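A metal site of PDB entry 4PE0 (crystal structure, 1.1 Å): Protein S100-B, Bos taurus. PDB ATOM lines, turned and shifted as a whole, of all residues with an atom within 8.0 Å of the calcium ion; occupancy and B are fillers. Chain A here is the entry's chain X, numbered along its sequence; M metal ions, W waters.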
ATOM      1  N   PHE A  15      -6.227   1.349 -14.715  1.00  0.00           N
ATOM      2  CA  PHE A  15      -6.617   2.512 -13.940  1.00  0.00           C
ATOM      3  C   PHE A  15      -7.177   3.564 -14.870  1.00  0.00           C
ATOM      4  O   PHE A  15      -8.274   4.108 -14.626  1.00  0.00           O
ATOM      5  CB  PHE A  15      -5.439   3.057 -13.152  1.00  0.00           C
ATOM      6  CG  PHE A  15      -5.777   4.330 -12.405  1.00  0.00           C
ATOM      7  CD1 PHE A  15      -6.474   4.277 -11.221  1.00  0.00           C
ATOM      8  CD2 PHE A  15      -5.416   5.572 -12.909  1.00  0.00           C
ATOM      9  CE1 PHE A  15      -6.803   5.445 -10.554  1.00  0.00           C
ATOM     10  CE2 PHE A  15      -5.719   6.724 -12.236  1.00  0.00           C
ATOM     11  CZ  PHE A  15      -6.416   6.666 -11.061  1.00  0.00           C
ATOM     12  N   HIS A  16      -6.479   3.845 -15.958  1.00  0.00           N
ATOM     13  CA  HIS A  16      -6.899   4.884 -16.879  1.00  0.00           C
ATOM     14  C   HIS A  16      -8.117   4.529 -17.706  1.00  0.00           C
ATOM     15  O   HIS A  16      -8.916   5.419 -18.049  1.00  0.00           O
ATOM     16  CB  HIS A  16      -5.762   5.228 -17.782  1.00  0.00           C
ATOM     17  CG  HIS A  16      -4.688   5.984 -17.098  1.00  0.00           C
ATOM     18  ND1 HIS A  16      -3.351   5.823 -17.411  1.00  0.00           N
ATOM     19  CD2 HIS A  16      -4.729   6.878 -16.082  1.00  0.00           C
ATOM     20  CE1 HIS A  16      -2.628   6.609 -16.628  1.00  0.00           C
ATOM     21  NE2 HIS A  16      -3.438   7.249 -15.811  1.00  0.00           N
ATOM     22  N   TYR A  18     -10.651   3.341 -16.594  1.00  0.00           N
ATOM     23  CA  TYR A  18     -11.777   3.696 -15.741  1.00  0.00           C
ATOM     24  C   TYR A  18     -11.708   5.143 -15.271  1.00  0.00           C
ATOM     25  O   TYR A  18     -12.754   5.823 -15.249  1.00  0.00           O
ATOM     26  CB  TYR A  18     -11.903   2.695 -14.576  1.00  0.00           C
ATOM     27  CG  TYR A  18     -12.457   1.398 -15.103  1.00  0.00           C
ATOM     28  CD1 TYR A  18     -11.628   0.424 -15.657  1.00  0.00           C
ATOM     29  CD2 TYR A  18     -13.821   1.171 -15.128  1.00  0.00           C
ATOM     30  CE1 TYR A  18     -12.151  -0.720 -16.210  1.00  0.00           C
ATOM     31  CE2 TYR A  18     -14.341   0.040 -15.654  1.00  0.00           C
ATOM     32  CZ  TYR A  18     -13.526  -0.902 -16.201  1.00  0.00           C
ATOM     33  OH  TYR A  18     -14.114  -2.015 -16.732  1.00  0.00           O
ATOM     34  N   SER A  19     -10.519   5.649 -14.961  1.00  0.00           N
ATOM     35  CA  SER A  19     -10.436   7.006 -14.433  1.00  0.00           C
ATOM     36  C   SER A  19     -10.794   8.049 -15.485  1.00  0.00           C
ATOM     37  O   SER A  19     -11.305   9.110 -15.157  1.00  0.00           O
ATOM     38  CB  SER A  19      -9.037   7.312 -13.875  1.00  0.00           C
ATOM     39  OG  SER A  19      -8.043   7.360 -14.884  1.00  0.00           O
ATOM     40  N   GLY A  20     -10.547   7.715 -16.741  1.00  0.00           N
ATOM     41  CA  GLY A  20     -10.725   8.644 -17.836  1.00  0.00           C
ATOM     42  C   GLY A  20     -12.159   8.774 -18.326  1.00  0.00           C
ATOM     43  O   GLY A  20     -12.429   9.555 -19.247  1.00  0.00           O
ATOM     44  N   ARG A  21     -13.089   8.083 -17.708  1.00  0.00           N
ATOM     45  CA  ARG A  21     -14.447   8.058 -18.246  1.00  0.00           C
ATOM     46  C   ARG A  21     -15.212   9.351 -17.999  1.00  0.00           C
ATOM     47  O   ARG A  21     -15.868   9.883 -18.922  1.00  0.00           O
ATOM     48  CB  ARG A  21     -15.229   6.896 -17.652  1.00  0.00           C
ATOM     49  CG  ARG A  21     -14.724   5.579 -18.129  1.00  0.00           C
ATOM     50  CD  ARG A  21     -15.387   4.472 -17.391  1.00  0.00           C
ATOM     51  NE  ARG A  21     -15.072   3.189 -17.997  1.00  0.00           N
ATOM     52  CZ  ARG A  21     -15.822   2.113 -17.835  1.00  0.00           C
ATOM     53  NH1 ARG A  21     -16.909   2.160 -17.072  1.00  0.00           N
ATOM     54  NH2 ARG A  21     -15.483   0.999 -18.440  1.00  0.00           N
ATOM     55  N   GLU A  22     -15.133   9.848 -16.783  1.00  0.00           N
ATOM     56  CA  GLU A  22     -15.932  10.983 -16.349  1.00  0.00           C
ATOM     57  C   GLU A  22     -15.160  11.847 -15.373  1.00  0.00           C
ATOM     58  O   GLU A  22     -14.200  11.378 -14.708  1.00  0.00           O
ATOM     59  CB  GLU A  22     -17.247  10.523 -15.713  1.00  0.00           C
ATOM     60  CG  GLU A  22     -18.266  10.043 -16.749  1.00  0.00           C
ATOM     61  CD  GLU A  22     -19.547   9.509 -16.144  1.00  0.00           C
ATOM     62  OE1 GLU A  22     -20.485   9.206 -16.916  1.00  0.00           O
ATOM     63  OE2 GLU A  22     -19.631   9.396 -14.903  1.00  0.00           O
ATOM     64  N   GLY A  23     -15.567  13.117 -15.297  1.00  0.00           N
ATOM     65  CA  GLY A  23     -14.964  14.002 -14.354  1.00  0.00           C
ATOM     66  C   GLY A  23     -13.473  14.135 -14.583  1.00  0.00           C
ATOM     67  O   GLY A  23     -13.003  14.166 -15.717  1.00  0.00           O
ATOM     68  N   ASP A  24     -12.715  14.223 -13.505  1.00  0.00           N
ATOM     69  CA  ASP A  24     -11.265  14.231 -13.621  1.00  0.00           C
ATOM     70  C   ASP A  24     -10.769  12.922 -14.237  1.00  0.00           C
ATOM     71  O   ASP A  24     -11.070  11.832 -13.725  1.00  0.00           O
ATOM     72  CB  ASP A  24     -10.665  14.388 -12.241  1.00  0.00           C
ATOM     73  CG  ASP A  24      -9.227  14.798 -12.294  1.00  0.00           C
ATOM     74  OD1 ASP A  24      -8.398  14.087 -12.906  1.00  0.00           O
ATOM     75  OD2 ASP A  24      -8.920  15.874 -11.747  1.00  0.00           O
ATOM     76  N   LYS A  25     -10.004  13.025 -15.315  1.00  0.00           N
ATOM     77  CA  LYS A  25      -9.552  11.837 -16.037  1.00  0.00           C
ATOM     78  C   LYS A  25      -8.481  11.053 -15.327  1.00  0.00           C
ATOM     79  O   LYS A  25      -8.157   9.933 -15.736  1.00  0.00           O
ATOM     80  CB  LYS A  25      -9.038  12.250 -17.419  1.00  0.00           C
ATOM     81  CG  LYS A  25     -10.110  12.692 -18.367  1.00  0.00           C
ATOM     82  CD  LYS A  25      -9.514  13.200 -19.658  1.00  0.00           C
ATOM     83  CE  LYS A  25     -10.591  13.573 -20.650  1.00  0.00           C
ATOM     84  NZ  LYS A  25     -10.026  14.179 -21.887  1.00  0.00           N
ATOM     85  N   HIS A  26      -7.926  11.629 -14.265  1.00  0.00           N
ATOM     86  CA  HIS A  26      -6.848  10.959 -13.514  1.00  0.00           C
ATOM     87  C   HIS A  26      -7.277  10.478 -12.125  1.00  0.00           C
ATOM     88  O   HIS A  26      -6.434  10.071 -11.325  1.00  0.00           O
ATOM     89  CB  HIS A  26      -5.638  11.876 -13.432  1.00  0.00           C
ATOM     90  CG  HIS A  26      -4.981  12.058 -14.749  1.00  0.00           C
ATOM     91  ND1 HIS A  26      -4.093  11.129 -15.251  1.00  0.00           N
ATOM     92  CD2 HIS A  26      -5.181  12.972 -15.733  1.00  0.00           C
ATOM     93  CE1 HIS A  26      -3.722  11.514 -16.461  1.00  0.00           C
ATOM     94  NE2 HIS A  26      -4.362  12.621 -16.770  1.00  0.00           N
ATOM     95  N   LYS A  27      -8.572  10.474 -11.853  1.00  0.00           N
ATOM     96  CA  LYS A  27      -9.075   9.912 -10.608  1.00  0.00           C
ATOM     97  C   LYS A  27     -10.297   9.092 -10.887  1.00  0.00           C
ATOM     98  O   LYS A  27     -11.035   9.391 -11.829  1.00  0.00           O
ATOM     99  CB  LYS A  27      -9.465  11.009  -9.629  1.00  0.00           C
ATOM    100  CG  LYS A  27      -8.333  11.938  -9.266  1.00  0.00           C
ATOM    101  CD  LYS A  27      -8.854  13.090  -8.430  1.00  0.00           C
ATOM    102  CE  LYS A  27      -7.773  14.118  -8.172  1.00  0.00           C
ATOM    103  NZ  LYS A  27      -8.329  15.328  -7.511  1.00  0.00           N
ATOM    104  N   LEU A  28     -10.510   8.072 -10.045  1.00  0.00           N
ATOM    105  CA  LEU A  28     -11.734   7.271 -10.073  1.00  0.00           C
ATOM    106  C   LEU A  28     -12.758   7.878  -9.133  1.00  0.00           C
ATOM    107  O   LEU A  28     -12.531   7.950  -7.943  1.00  0.00           O
ATOM    108  CB  LEU A  28     -11.455   5.859  -9.591  1.00  0.00           C
ATOM    109  CG  LEU A  28     -10.452   5.052 -10.391  1.00  0.00           C
ATOM    110  CD1 LEU A  28      -9.952   3.847  -9.603  1.00  0.00           C
ATOM    111  CD2 LEU A  28     -11.026   4.575 -11.696  1.00  0.00           C
ATOM    112  N   LYS A  29     -13.862   8.340  -9.694  1.00  0.00           N
ATOM    113  CA  LYS A  29     -15.012   8.678  -8.864  1.00  0.00           C
ATOM    114  C   LYS A  29     -15.732   7.381  -8.487  1.00  0.00           C
ATOM    115  O   LYS A  29     -15.372   6.305  -8.944  1.00  0.00           O
ATOM    116  CB  LYS A  29     -15.954   9.635  -9.594  1.00  0.00           C
ATOM    117  CG  LYS A  29     -16.626   9.046 -10.811  1.00  0.00           C
ATOM    118  CD  LYS A  29     -17.398  10.078 -11.614  1.00  0.00           C
ATOM    119  CE  LYS A  29     -18.708  10.427 -10.961  1.00  0.00           C
ATOM    120  NZ  LYS A  29     -19.797   9.522 -11.407  1.00  0.00           N
ATOM    121  N   LYS A  30     -16.728   7.484  -7.613  1.00  0.00           N
ATOM    122  CA  LYS A  30     -17.379   6.291  -7.092  1.00  0.00           C
ATOM    123  C   LYS A  30     -17.884   5.382  -8.198  1.00  0.00           C
ATOM    124  O   LYS A  30     -17.672   4.189  -8.154  1.00  0.00           O
ATOM    125  CB  LYS A  30     -18.487   6.672  -6.095  1.00  0.00           C
ATOM    126  CG  LYS A  30     -17.906   7.129  -4.803  1.00  0.00           C
ATOM    127  CD  LYS A  30     -18.943   7.699  -3.831  1.00  0.00           C
ATOM    128  CE  LYS A  30     -18.256   8.054  -2.515  1.00  0.00           C
ATOM    129  NZ  LYS A  30     -17.280   9.173  -2.625  1.00  0.00           N
ATOM    130  N   SER A  31     -18.551   5.929  -9.207  1.00  0.00           N
ATOM    131  CA  SER A  31     -19.097   5.079 -10.251  1.00  0.00           C
ATOM    132  C   SER A  31     -18.006   4.368 -11.062  1.00  0.00           C
ATOM    133  O   SER A  31     -18.188   3.215 -11.465  1.00  0.00           O
ATOM    134  CB  SER A  31     -20.004   5.880 -11.184  1.00  0.00           C
ATOM    135  OG  SER A  31     -19.277   6.897 -11.834  1.00  0.00           O
ATOM    136  N   GLU A  32     -16.881   5.038 -11.287  1.00  0.00           N
ATOM    137  CA  GLU A  32     -15.768   4.467 -12.026  1.00  0.00           C
ATOM    138  C   GLU A  32     -15.121   3.353 -11.227  1.00  0.00           C
ATOM    139  O   GLU A  32     -14.757   2.307 -11.780  1.00  0.00           O
ATOM    140  CB  GLU A  32     -14.737   5.544 -12.355  1.00  0.00           C
ATOM    141  CG  GLU A  32     -15.229   6.553 -13.391  1.00  0.00           C
ATOM    142  CD  GLU A  32     -14.319   7.777 -13.495  1.00  0.00           C
ATOM    143  OE1 GLU A  32     -13.626   8.106 -12.527  1.00  0.00           O
ATOM    144  OE2 GLU A  32     -14.309   8.440 -14.566  1.00  0.00           O
ATOM    145  N   LEU A  33     -14.952   3.549  -9.928  1.00  0.00           N
ATOM    146  CA  LEU A  33     -14.394   2.547  -9.059  1.00  0.00           C
ATOM    147  C   LEU A  33     -15.293   1.310  -9.017  1.00  0.00           C
ATOM    148  O   LEU A  33     -14.833   0.174  -9.054  1.00  0.00           O
ATOM    149  CB  LEU A  33     -14.217   3.118  -7.651  1.00  0.00           C
ATOM    150  CG  LEU A  33     -13.670   2.165  -6.590  1.00  0.00           C
ATOM    151  CD1 LEU A  33     -12.297   1.651  -6.971  1.00  0.00           C
ATOM    152  CD2 LEU A  33     -13.686   2.823  -5.193  1.00  0.00           C
ATOM    153  N   GLU A  68     -12.224  10.841  -4.060  1.00  0.00           N
ATOM    154  CA  GLU A  68     -12.001   9.969  -5.214  1.00  0.00           C
ATOM    155  C   GLU A  68     -10.745   9.165  -5.003  1.00  0.00           C
ATOM    156  O   GLU A  68     -10.027   9.390  -4.040  1.00  0.00           O
ATOM    157  CB  GLU A  68     -11.893  10.792  -6.499  1.00  0.00           C
ATOM    158  CG  GLU A  68     -13.131  11.642  -6.790  1.00  0.00           C
ATOM    159  CD  GLU A  68     -13.268  12.082  -8.243  1.00  0.00           C
ATOM    160  OE1 GLU A  68     -12.668  11.449  -9.141  1.00  0.00           O
ATOM    161  OE2 GLU A  68     -13.982  13.085  -8.482  1.00  0.00           O
ATOM    162  N   CYS A  69     -10.498   8.218  -5.893  1.00  0.00           N
ATOM    163  CA  CYS A  69      -9.332   7.356  -5.794  1.00  0.00           C
ATOM    164  C   CYS A  69      -8.338   7.698  -6.889  1.00  0.00           C
ATOM    165  O   CYS A  69      -8.611   7.499  -8.056  1.00  0.00           O
ATOM    166  CB  CYS A  69      -9.771   5.897  -5.906  1.00  0.00           C
ATOM    167  SG  CYS A  69      -8.448   4.677  -5.709  1.00  0.00           S
HETATM  168 CA    CA M   1     -12.643  10.064 -13.450  1.00  0.00          CA
HETATM  169  O   HOH W   1     -13.541  11.196 -11.583  1.00  0.00           O
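Water W1 binds the calcium ion, at 2.4 Å.
The calcium ion is bound by the backbone carbonyl oxygen (O) of Ser 19 (2.4 Å).
OE1 of Glu 32 is bound to the calcium ion, 2.4 Å away.
The backbone carbonyl oxygen (O) of Lys 27 binds the calcium ion.
O of Asp 24 is bound to the calcium ion.
O of Glu 22 is bound to the calcium ion, at 2.4 Å.
The side-chain carboxylate (OE2) of Glu 32 is bound to the calcium ion (2.6 Å).
The calcium ion has seven donor atoms within binding distance.
Water W1 bridges the side-chain carboxylate of Glu 68 (2.6 Å) and the backbone NH of Lys 29 (3.4 Å).
The side-chain carboxylate of Glu 32 lies close to the backbone NH of Lys 29, at 2.9 Å.
The side-chain carboxylate (OE2) of Glu 32 sits close to the backbone NH (N) of Arg 21 (3.4 Å).
OG of Ser 19 sits at hydrogen-bond distance from O of Lys 25, 2.7 Å away.
The side-chain hydroxyl of Ser 19 sits at hydrogen-bond distance from the backbone carbonyl oxygen of Phe 15 (3.3 Å).
NZ of Lys 29 lies within salt-bridge range of OE2 of Glu 22 (3.5 Å).
The side-chain carboxylate of Asp 24 sits at hydrogen-bond distance from the backbone NH of His 26 (2.8 Å).
Of the 20 residues printed, 5 come within 4 Å of the calcium ion.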
